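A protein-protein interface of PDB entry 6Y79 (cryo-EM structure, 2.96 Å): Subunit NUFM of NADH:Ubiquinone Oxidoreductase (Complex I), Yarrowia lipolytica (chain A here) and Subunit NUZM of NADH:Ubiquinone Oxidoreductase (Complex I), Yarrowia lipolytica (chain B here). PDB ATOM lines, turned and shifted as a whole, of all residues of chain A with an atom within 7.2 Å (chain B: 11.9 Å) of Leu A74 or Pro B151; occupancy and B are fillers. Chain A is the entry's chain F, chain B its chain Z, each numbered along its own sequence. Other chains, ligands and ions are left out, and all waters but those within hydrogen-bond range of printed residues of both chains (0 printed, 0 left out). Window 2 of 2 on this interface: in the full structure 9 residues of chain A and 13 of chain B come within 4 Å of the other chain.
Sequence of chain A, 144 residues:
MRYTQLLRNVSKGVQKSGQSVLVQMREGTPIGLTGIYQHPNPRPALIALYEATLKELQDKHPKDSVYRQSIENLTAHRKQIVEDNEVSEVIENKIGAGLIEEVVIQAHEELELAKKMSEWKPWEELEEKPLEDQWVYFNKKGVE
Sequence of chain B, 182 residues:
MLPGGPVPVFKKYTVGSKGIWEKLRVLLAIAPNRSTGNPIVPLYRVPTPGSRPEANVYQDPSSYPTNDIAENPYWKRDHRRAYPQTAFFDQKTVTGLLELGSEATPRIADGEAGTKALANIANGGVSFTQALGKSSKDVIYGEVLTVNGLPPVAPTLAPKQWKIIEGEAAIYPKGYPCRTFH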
ATOM      1  N   TYR A  50      16.509 -16.119   5.604  1.00  0.00           N
ATOM      2  CA  TYR A  50      16.561 -17.216   6.571  1.00  0.00           C
ATOM      3  C   TYR A  50      17.945 -17.846   6.639  1.00  0.00           C
ATOM      4  O   TYR A  50      18.458 -18.129   7.730  1.00  0.00           O
ATOM      5  CB  TYR A  50      15.544 -18.290   6.200  1.00  0.00           C
ATOM      6  CG  TYR A  50      14.100 -17.934   6.415  1.00  0.00           C
ATOM      7  CD1 TYR A  50      13.726 -16.873   7.230  1.00  0.00           C
ATOM      8  CD2 TYR A  50      13.105 -18.673   5.800  1.00  0.00           C
ATOM      9  CE1 TYR A  50      12.398 -16.564   7.422  1.00  0.00           C
ATOM     10  CE2 TYR A  50      11.781 -18.377   5.986  1.00  0.00           C
ATOM     11  CZ  TYR A  50      11.433 -17.322   6.798  1.00  0.00           C
ATOM     12  OH  TYR A  50      10.105 -17.026   6.977  1.00  0.00           O
ATOM     13  N   LEU A  54      20.548 -18.123   9.811  1.00  0.00           N
ATOM     14  CA  LEU A  54      21.056 -19.375  10.368  1.00  0.00           C
ATOM     15  C   LEU A  54      22.580 -19.447  10.300  1.00  0.00           C
ATOM     16  O   LEU A  54      23.225 -19.913  11.246  1.00  0.00           O
ATOM     17  CB  LEU A  54      20.428 -20.569   9.651  1.00  0.00           C
ATOM     18  CG  LEU A  54      18.997 -20.911  10.072  1.00  0.00           C
ATOM     19  CD1 LEU A  54      18.493 -22.107   9.290  1.00  0.00           C
ATOM     20  CD2 LEU A  54      18.909 -21.177  11.564  1.00  0.00           C
ATOM     21  N   VAL A  66      20.330 -20.446  25.089  1.00  0.00           N
ATOM     22  CA  VAL A  66      18.911 -20.676  24.864  1.00  0.00           C
ATOM     23  C   VAL A  66      18.418 -19.819  23.705  1.00  0.00           C
ATOM     24  O   VAL A  66      17.578 -20.249  22.897  1.00  0.00           O
ATOM     25  CB  VAL A  66      18.161 -20.399  26.174  1.00  0.00           C
ATOM     26  CG1 VAL A  66      16.702 -20.610  25.998  1.00  0.00           C
ATOM     27  CG2 VAL A  66      18.685 -21.315  27.268  1.00  0.00           C
ATOM     28  N   ARG A  68      20.210 -18.831  21.001  1.00  0.00           N
ATOM     29  CA  ARG A  68      20.652 -19.433  19.748  1.00  0.00           C
ATOM     30  C   ARG A  68      19.831 -20.665  19.396  1.00  0.00           C
ATOM     31  O   ARG A  68      19.408 -20.811  18.246  1.00  0.00           O
ATOM     32  CB  ARG A  68      22.135 -19.783  19.844  1.00  0.00           C
ATOM     33  CG  ARG A  68      22.739 -20.468  18.621  1.00  0.00           C
ATOM     34  CD  ARG A  68      24.114 -20.970  18.979  1.00  0.00           C
ATOM     35  NE  ARG A  68      24.959 -21.436  17.883  1.00  0.00           N
ATOM     36  CZ  ARG A  68      24.998 -22.692  17.452  1.00  0.00           C
ATOM     37  NH1 ARG A  68      24.221 -23.609  18.007  1.00  0.00           N
ATOM     38  NH2 ARG A  68      25.810 -23.037  16.466  1.00  0.00           N
ATOM     39  N   GLN A  69      19.574 -21.541  20.380  1.00  0.00           N
ATOM     40  CA  GLN A  69      18.790 -22.759  20.151  1.00  0.00           C
ATOM     41  C   GLN A  69      17.391 -22.434  19.652  1.00  0.00           C
ATOM     42  O   GLN A  69      16.906 -23.029  18.678  1.00  0.00           O
ATOM     43  CB  GLN A  69      18.692 -23.583  21.437  1.00  0.00           C
ATOM     44  CG  GLN A  69      19.910 -24.387  21.811  1.00  0.00           C
ATOM     45  CD  GLN A  69      19.760 -25.018  23.172  1.00  0.00           C
ATOM     46  OE1 GLN A  69      18.665 -25.057  23.726  1.00  0.00           O
ATOM     47  NE2 GLN A  69      20.869 -25.464  23.745  1.00  0.00           N
ATOM     48  N   SER A  70      16.751 -21.443  20.273  1.00  0.00           N
ATOM     49  CA  SER A  70      15.389 -21.101  19.893  1.00  0.00           C
ATOM     50  C   SER A  70      15.297 -20.415  18.540  1.00  0.00           C
ATOM     51  O   SER A  70      14.389 -20.733  17.769  1.00  0.00           O
ATOM     52  CB  SER A  70      14.764 -20.208  20.948  1.00  0.00           C
ATOM     53  OG  SER A  70      15.267 -18.888  20.846  1.00  0.00           O
ATOM     54  N   ILE A  71      16.197 -19.480  18.220  1.00  0.00           N
ATOM     55  CA  ILE A  71      16.064 -18.845  16.910  1.00  0.00           C
ATOM     56  C   ILE A  71      16.540 -19.782  15.791  1.00  0.00           C
ATOM     57  O   ILE A  71      16.031 -19.702  14.663  1.00  0.00           O
ATOM     58  CB  ILE A  71      16.767 -17.476  16.908  1.00  0.00           C
ATOM     59  CG1 ILE A  71      16.278 -16.676  18.115  1.00  0.00           C
ATOM     60  CG2 ILE A  71      16.470 -16.693  15.630  1.00  0.00           C
ATOM     61  CD1 ILE A  71      16.497 -15.183  18.049  1.00  0.00           C
ATOM     62  N   GLU A  72      17.441 -20.728  16.102  1.00  0.00           N
ATOM     63  CA  GLU A  72      17.734 -21.848  15.208  1.00  0.00           C
ATOM     64  C   GLU A  72      16.479 -22.623  14.852  1.00  0.00           C
ATOM     65  O   GLU A  72      16.140 -22.749  13.670  1.00  0.00           O
ATOM     66  CB  GLU A  72      18.748 -22.799  15.846  1.00  0.00           C
ATOM     67  CG  GLU A  72      20.188 -22.474  15.550  1.00  0.00           C
ATOM     68  CD  GLU A  72      21.149 -23.584  15.889  1.00  0.00           C
ATOM     69  OE1 GLU A  72      21.670 -23.580  17.028  1.00  0.00           O
ATOM     70  OE2 GLU A  72      21.432 -24.438  15.016  1.00  0.00           O
ATOM     71  N   ASN A  73      15.781 -23.146  15.870  1.00  0.00           N
ATOM     72  CA  ASN A  73      14.596 -23.965  15.626  1.00  0.00           C
ATOM     73  C   ASN A  73      13.477 -23.158  14.982  1.00  0.00           C
ATOM     74  O   ASN A  73      12.718 -23.678  14.158  1.00  0.00           O
ATOM     75  CB  ASN A  73      14.121 -24.567  16.937  1.00  0.00           C
ATOM     76  CG  ASN A  73      15.141 -25.484  17.560  1.00  0.00           C
ATOM     77  OD1 ASN A  73      15.726 -26.325  16.888  1.00  0.00           O
ATOM     78  ND2 ASN A  73      15.363 -25.324  18.860  1.00  0.00           N
ATOM     79  N   LEU A  74      13.398 -21.870  15.305  1.00  0.00           N
ATOM     80  CA  LEU A  74      12.329 -21.029  14.790  1.00  0.00           C
ATOM     81  C   LEU A  74      12.508 -20.731  13.307  1.00  0.00           C
ATOM     82  O   LEU A  74      11.575 -20.912  12.510  1.00  0.00           O
ATOM     83  CB  LEU A  74      12.293 -19.741  15.586  1.00  0.00           C
ATOM     84  CG  LEU A  74      11.211 -18.793  15.140  1.00  0.00           C
ATOM     85  CD1 LEU A  74       9.878 -19.436  15.397  1.00  0.00           C
ATOM     86  CD2 LEU A  74      11.392 -17.598  15.990  1.00  0.00           C
ATOM     87  N   THR A  75      13.699 -20.256  12.921  1.00  0.00           N
ATOM     88  CA  THR A  75      13.969 -20.000  11.514  1.00  0.00           C
ATOM     89  C   THR A  75      14.012 -21.289  10.704  1.00  0.00           C
ATOM     90  O   THR A  75      13.631 -21.270   9.533  1.00  0.00           O
ATOM     91  CB  THR A  75      15.274 -19.212  11.376  1.00  0.00           C
ATOM     92  OG1 THR A  75      15.314 -18.195  12.380  1.00  0.00           O
ATOM     93  CG2 THR A  75      15.369 -18.539  10.021  1.00  0.00           C
ATOM     94  N   ALA A  76      14.387 -22.416  11.323  1.00  0.00           N
ATOM     95  CA  ALA A  76      14.307 -23.706  10.644  1.00  0.00           C
ATOM     96  C   ALA A  76      12.864 -24.109  10.367  1.00  0.00           C
ATOM     97  O   ALA A  76      12.555 -24.612   9.281  1.00  0.00           O
ATOM     98  CB  ALA A  76      15.008 -24.776  11.479  1.00  0.00           C
ATOM     99  N   HIS A  77      11.965 -23.871  11.327  1.00  0.00           N
ATOM    100  CA  HIS A  77      10.549 -24.182  11.146  1.00  0.00           C
ATOM    101  C   HIS A  77       9.923 -23.310  10.063  1.00  0.00           C
ATOM    102  O   HIS A  77       9.195 -23.807   9.188  1.00  0.00           O
ATOM    103  CB  HIS A  77       9.827 -23.996  12.480  1.00  0.00           C
ATOM    104  CG  HIS A  77       8.410 -24.472  12.482  1.00  0.00           C
ATOM    105  ND1 HIS A  77       7.366 -23.701  12.019  1.00  0.00           N
ATOM    106  CD2 HIS A  77       7.860 -25.630  12.913  1.00  0.00           C
ATOM    107  CE1 HIS A  77       6.236 -24.370  12.153  1.00  0.00           C
ATOM    108  NE2 HIS A  77       6.507 -25.543  12.693  1.00  0.00           N
ATOM    109  N   ARG A  78      10.222 -22.008  10.097  1.00  0.00           N
ATOM    110  CA  ARG A  78       9.689 -21.092   9.092  1.00  0.00           C
ATOM    111  C   ARG A  78      10.242 -21.402   7.708  1.00  0.00           C
ATOM    112  O   ARG A  78       9.503 -21.370   6.720  1.00  0.00           O
ATOM    113  CB  ARG A  78       9.991 -19.645   9.476  1.00  0.00           C
ATOM    114  CG  ARG A  78       9.015 -19.055  10.475  1.00  0.00           C
ATOM    115  CD  ARG A  78       9.440 -17.671  10.934  1.00  0.00           C
ATOM    116  NE  ARG A  78       8.682 -17.261  12.111  1.00  0.00           N
ATOM    117  CZ  ARG A  78       7.721 -16.347  12.107  1.00  0.00           C
ATOM    118  NH1 ARG A  78       7.401 -15.723  10.987  1.00  0.00           N
ATOM    119  NH2 ARG A  78       7.087 -16.052  13.227  1.00  0.00           N
ATOM    120  N   LYS A  79      11.533 -21.738   7.623  1.00  0.00           N
ATOM    121  CA  LYS A  79      12.154 -22.088   6.352  1.00  0.00           C
ATOM    122  C   LYS A  79      11.593 -23.380   5.782  1.00  0.00           C
ATOM    123  O   LYS A  79      11.419 -23.492   4.561  1.00  0.00           O
ATOM    124  CB  LYS A  79      13.661 -22.199   6.552  1.00  0.00           C
ATOM    125  CG  LYS A  79      14.473 -22.347   5.293  1.00  0.00           C
ATOM    126  CD  LYS A  79      15.951 -22.344   5.628  1.00  0.00           C
ATOM    127  CE  LYS A  79      16.783 -22.643   4.405  1.00  0.00           C
ATOM    128  NZ  LYS A  79      16.468 -23.975   3.824  1.00  0.00           N
ATOM    129  N   GLN A  80      11.288 -24.349   6.651  1.00  0.00           N
ATOM    130  CA  GLN A  80      10.643 -25.580   6.210  1.00  0.00           C
ATOM    131  C   GLN A  80       9.261 -25.305   5.633  1.00  0.00           C
ATOM    132  O   GLN A  80       8.906 -25.849   4.576  1.00  0.00           O
ATOM    133  CB  GLN A  80      10.553 -26.560   7.377  1.00  0.00           C
ATOM    134  CG  GLN A  80       9.895 -27.877   7.038  1.00  0.00           C
ATOM    135  CD  GLN A  80       9.869 -28.828   8.213  1.00  0.00           C
ATOM    136  OE1 GLN A  80      10.256 -28.472   9.326  1.00  0.00           O
ATOM    137  NE2 GLN A  80       9.416 -30.052   7.971  1.00  0.00           N
ATOM    138  N   GLU A 110      14.802  -9.901  12.613  1.00  0.00           N
ATOM    139  CA  GLU A 110      15.490 -10.888  13.439  1.00  0.00           C
ATOM    140  C   GLU A 110      16.920 -11.123  12.963  1.00  0.00           C
ATOM    141  O   GLU A 110      17.786 -11.455  13.780  1.00  0.00           O
ATOM    142  CB  GLU A 110      14.709 -12.203  13.486  1.00  0.00           C
ATOM    143  CG  GLU A 110      14.715 -12.991  12.201  1.00  0.00           C
ATOM    144  CD  GLU A 110      14.185 -14.391  12.350  1.00  0.00           C
ATOM    145  OE1 GLU A 110      14.768 -15.161  13.139  1.00  0.00           O
ATOM    146  OE2 GLU A 110      13.191 -14.725  11.671  1.00  0.00           O
ATOM    147  N   ILE B 140      15.610 -28.311  29.085  1.00  0.00           N
ATOM    148  CA  ILE B 140      15.640 -27.052  28.348  1.00  0.00           C
ATOM    149  C   ILE B 140      14.482 -27.003  27.362  1.00  0.00           C
ATOM    150  O   ILE B 140      13.823 -25.970  27.202  1.00  0.00           O
ATOM    151  CB  ILE B 140      17.010 -26.849  27.664  1.00  0.00           C
ATOM    152  CG1 ILE B 140      18.071 -26.459  28.689  1.00  0.00           C
ATOM    153  CG2 ILE B 140      16.976 -25.749  26.630  1.00  0.00           C
ATOM    154  CD1 ILE B 140      19.490 -26.543  28.155  1.00  0.00           C
ATOM    155  N   TYR B 141      14.156 -28.134  26.757  1.00  0.00           N
ATOM    156  CA  TYR B 141      13.040 -28.201  25.830  1.00  0.00           C
ATOM    157  C   TYR B 141      11.715 -28.475  26.520  1.00  0.00           C
ATOM    158  O   TYR B 141      10.678 -28.455  25.855  1.00  0.00           O
ATOM    159  CB  TYR B 141      13.286 -29.278  24.767  1.00  0.00           C
ATOM    160  CG  TYR B 141      14.378 -28.947  23.774  1.00  0.00           C
ATOM    161  CD1 TYR B 141      14.900 -27.665  23.680  1.00  0.00           C
ATOM    162  CD2 TYR B 141      14.881 -29.920  22.923  1.00  0.00           C
ATOM    163  CE1 TYR B 141      15.897 -27.363  22.781  1.00  0.00           C
ATOM    164  CE2 TYR B 141      15.879 -29.625  22.013  1.00  0.00           C
ATOM    165  CZ  TYR B 141      16.381 -28.344  21.948  1.00  0.00           C
ATOM    166  OH  TYR B 141      17.374 -28.043  21.046  1.00  0.00           O
ATOM    167  N   GLY B 142      11.718 -28.749  27.821  1.00  0.00           N
ATOM    168  CA  GLY B 142      10.471 -28.964  28.528  1.00  0.00           C
ATOM    169  C   GLY B 142       9.954 -27.750  29.276  1.00  0.00           C
ATOM    170  O   GLY B 142       8.792 -27.372  29.117  1.00  0.00           O
ATOM    171  N   GLU B 143      10.810 -27.124  30.082  1.00  0.00           N
ATOM    172  CA  GLU B 143      10.423 -26.009  30.932  1.00  0.00           C
ATOM    173  C   GLU B 143      10.821 -24.646  30.401  1.00  0.00           C
ATOM    174  O   GLU B 143      10.090 -23.678  30.631  1.00  0.00           O
ATOM    175  CB  GLU B 143      11.020 -26.172  32.335  1.00  0.00           C
ATOM    176  CG  GLU B 143      10.538 -27.411  33.055  1.00  0.00           C
ATOM    177  CD  GLU B 143      10.743 -27.342  34.552  1.00  0.00           C
ATOM    178  OE1 GLU B 143      11.681 -26.652  34.995  1.00  0.00           O
ATOM    179  OE2 GLU B 143       9.967 -27.992  35.283  1.00  0.00           O
ATOM    180  N   VAL B 144      11.955 -24.533  29.713  1.00  0.00           N
ATOM    181  CA  VAL B 144      12.355 -23.235  29.190  1.00  0.00           C
ATOM    182  C   VAL B 144      11.705 -22.978  27.840  1.00  0.00           C
ATOM    183  O   VAL B 144      11.138 -21.908  27.600  1.00  0.00           O
ATOM    184  CB  VAL B 144      13.884 -23.152  29.103  1.00  0.00           C
ATOM    185  CG1 VAL B 144      14.288 -21.843  28.491  1.00  0.00           C
ATOM    186  CG2 VAL B 144      14.513 -23.299  30.473  1.00  0.00           C
ATOM    187  N   LEU B 145      11.754 -23.958  26.950  1.00  0.00           N
ATOM    188  CA  LEU B 145      11.216 -23.831  25.608  1.00  0.00           C
ATOM    189  C   LEU B 145       9.913 -24.609  25.480  1.00  0.00           C
ATOM    190  O   LEU B 145       9.437 -25.245  26.422  1.00  0.00           O
ATOM    191  CB  LEU B 145      12.219 -24.333  24.566  1.00  0.00           C
ATOM    192  CG  LEU B 145      13.391 -23.494  24.055  1.00  0.00           C
ATOM    193  CD1 LEU B 145      14.434 -23.351  25.096  1.00  0.00           C
ATOM    194  CD2 LEU B 145      14.011 -24.193  22.895  1.00  0.00           C
ATOM    195  N   THR B 146       9.331 -24.538  24.287  1.00  0.00           N
ATOM    196  CA  THR B 146       8.220 -25.396  23.904  1.00  0.00           C
ATOM    197  C   THR B 146       8.733 -26.833  23.759  1.00  0.00           C
ATOM    198  O   THR B 146       9.916 -27.062  23.488  1.00  0.00           O
ATOM    199  CB  THR B 146       7.599 -24.851  22.605  1.00  0.00           C
ATOM    200  OG1 THR B 146       7.212 -23.489  22.821  1.00  0.00           O
ATOM    201  CG2 THR B 146       6.357 -25.611  22.108  1.00  0.00           C
ATOM    202  N   VAL B 147       7.827 -27.806  23.926  1.00  0.00           N
ATOM    203  CA  VAL B 147       8.154 -29.216  23.784  1.00  0.00           C
ATOM    204  C   VAL B 147       8.660 -29.577  22.381  1.00  0.00           C
ATOM    205  O   VAL B 147       9.261 -30.641  22.201  1.00  0.00           O
ATOM    206  CB  VAL B 147       6.921 -30.050  24.166  1.00  0.00           C
ATOM    207  CG1 VAL B 147       6.348 -29.543  25.479  1.00  0.00           C
ATOM    208  CG2 VAL B 147       5.867 -30.003  23.077  1.00  0.00           C
ATOM    209  N   ASN B 148       8.434 -28.731  21.372  1.00  0.00           N
ATOM    210  CA  ASN B 148       9.003 -28.915  20.043  1.00  0.00           C
ATOM    211  C   ASN B 148      10.327 -28.189  19.857  1.00  0.00           C
ATOM    212  O   ASN B 148      10.952 -28.328  18.800  1.00  0.00           O
ATOM    213  CB  ASN B 148       8.003 -28.450  18.990  1.00  0.00           C
ATOM    214  CG  ASN B 148       6.714 -29.235  19.047  1.00  0.00           C
ATOM    215  OD1 ASN B 148       5.656 -28.691  19.358  1.00  0.00           O
ATOM    216  ND2 ASN B 148       6.796 -30.527  18.758  1.00  0.00           N
ATOM    217  N   GLY B 149      10.762 -27.421  20.847  1.00  0.00           N
ATOM    218  CA  GLY B 149      12.004 -26.692  20.767  1.00  0.00           C
ATOM    219  C   GLY B 149      11.886 -25.282  20.253  1.00  0.00           C
ATOM    220  O   GLY B 149      12.904 -24.691  19.897  1.00  0.00           O
ATOM    221  N   LEU B 150      10.723 -24.742  20.208  1.00  0.00           N
ATOM    222  CA  LEU B 150      10.456 -23.419  19.675  1.00  0.00           C
ATOM    223  C   LEU B 150      10.321 -22.411  20.811  1.00  0.00           C
ATOM    224  O   LEU B 150      10.043 -22.796  21.948  1.00  0.00           O
ATOM    225  CB  LEU B 150       9.178 -23.454  18.833  1.00  0.00           C
ATOM    226  CG  LEU B 150       9.359 -24.355  17.613  1.00  0.00           C
ATOM    227  CD1 LEU B 150       8.035 -24.755  16.999  1.00  0.00           C
ATOM    228  CD2 LEU B 150      10.244 -23.666  16.594  1.00  0.00           C
ATOM    229  N   PRO B 151      10.556 -21.115  20.585  1.00  0.00           N
ATOM    230  CA  PRO B 151      10.324 -20.149  21.654  1.00  0.00           C
ATOM    231  C   PRO B 151       8.837 -19.964  21.888  1.00  0.00           C
ATOM    232  O   PRO B 151       8.030 -20.086  20.951  1.00  0.00           O
ATOM    233  CB  PRO B 151      10.973 -18.861  21.115  1.00  0.00           C
ATOM    234  CG  PRO B 151      10.943 -19.011  19.660  1.00  0.00           C
ATOM    235  CD  PRO B 151      11.141 -20.475  19.394  1.00  0.00           C
ATOM    236  N   PRO B 152       8.422 -19.706  23.127  1.00  0.00           N
ATOM    237  CA  PRO B 152       6.999 -19.486  23.381  1.00  0.00           C
ATOM    238  C   PRO B 152       6.573 -18.125  22.869  1.00  0.00           C
ATOM    239  O   PRO B 152       7.294 -17.136  22.997  1.00  0.00           O
ATOM    240  CB  PRO B 152       6.893 -19.576  24.905  1.00  0.00           C
ATOM    241  CG  PRO B 152       8.206 -19.168  25.382  1.00  0.00           C
ATOM    242  CD  PRO B 152       9.209 -19.636  24.367  1.00  0.00           C
ATOM    243  N   VAL B 153       5.399 -18.090  22.250  1.00  0.00           N
ATOM    244  CA  VAL B 153       4.919 -16.849  21.667  1.00  0.00           C
ATOM    245  C   VAL B 153       4.318 -15.990  22.773  1.00  0.00           C
ATOM    246  O   VAL B 153       3.854 -16.511  23.799  1.00  0.00           O
ATOM    247  CB  VAL B 153       3.929 -17.162  20.526  1.00  0.00           C
ATOM    248  CG1 VAL B 153       2.613 -17.710  21.043  1.00  0.00           C
ATOM    249  CG2 VAL B 153       3.706 -15.967  19.655  1.00  0.00           C
ATOM    250  N   ALA B 154       4.412 -14.659  22.609  1.00  0.00           N
ATOM    251  CA  ALA B 154       3.901 -13.656  23.539  1.00  0.00           C
ATOM    252  C   ALA B 154       2.414 -13.865  23.777  1.00  0.00           C
ATOM    253  O   ALA B 154       1.605 -13.716  22.853  1.00  0.00           O
ATOM    254  CB  ALA B 154       4.160 -12.247  23.013  1.00  0.00           C
ATOM    255  N   PRO B 155       2.022 -14.219  24.997  1.00  0.00           N
ATOM    256  CA  PRO B 155       0.665 -14.722  25.219  1.00  0.00           C
ATOM    257  C   PRO B 155      -0.367 -13.608  25.251  1.00  0.00           C
ATOM    258  O   PRO B 155      -0.107 -12.496  25.713  1.00  0.00           O
ATOM    259  CB  PRO B 155       0.778 -15.417  26.580  1.00  0.00           C
ATOM    260  CG  PRO B 155       1.840 -14.663  27.277  1.00  0.00           C
ATOM    261  CD  PRO B 155       2.811 -14.189  26.239  1.00  0.00           C
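The backbone carbonyl oxygen of Ile B140 sits at hydrogen-bond distance from the backbone NH of Leu B145, 2.9 Å away. The side-chain hydroxyl of Thr B146 is in hydrogen-bond range of the backbone carbonyl oxygen of Leu B150, 3.0 Å away. The side-chain hydroxyl (OG) of Ser A70 lies within hydrogen-bond range of the backbone carbonyl oxygen (O) of Val A66 (3.4 Å). O of Gln A69 is in hydrogen-bond range of ND2 of Asn A73.
ND2 of Asn A73 lies within hydrogen-bond range of O of Gly B149 (2.7 Å).
Of the 16 printed residues of chain B, 7 touch a printed residue of chain A. Printed residues of chain A that touch a printed residue of chain B: Val A66, Gln A69, Ser A70, Asn A73 and Leu A74. Among the printed residues, 9 pairs touch across the chains. Among the printed residues, no Asp or Glu carboxylate lies within 4 Å of a Lys or Arg side-chain nitrogen of the other chain.
Among the printed residues, merely in contact across the chains: Val A66 with Val B144 (3.7 Å), Val A66 with Leu B145 (3.7 Å), Gln A69 with Ile B140 (3.4 Å), Gln A69 with Tyr B141 (3.7 Å), Ser A70 with Pro B151 (3.6 Å), Asn A73 with Leu B150 (3.5 Å), Leu A74 with Leu B150 (3.8 Å) and Leu A74 with Pro B151 (3.96 Å).
Of chain B, only Pro B151 (3.6 Å) comes within 4 Å of Ser A70. No residue of chain B comes within 4 Å of Ile A71. Asn A73 touches just these residues of chain B: Gly B149 (2.7 Å) and Leu B150 (3.5 Å). Leu A74 touches just these residues of chain B: Leu B150 and Pro B151. No residue of chain B comes within 4 Å of Thr A75. No residue of chain B comes within 4 Å of Ala A76. No residue of chain B comes within 4 Å of His A77. No residue of chain B comes within 4 Å of Arg A78. Gln A80 touches none of the printed residues of chain B. Printed residues of chain A within 4 Å of Ile B140: Gln A69 (3.4 Å). Printed residues of chain A within 4 Å of Val B144: Val A66. Of chain A, only Ser A70 and Leu A74 come within 4 Å of Pro B151. The nearest residue of chain A that does not touch Pro B151 is Ile A71 (5.3 Å). The nearest printed residue of chain A that does not touch Tyr B141 is Asn A73 (4.03 Å).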
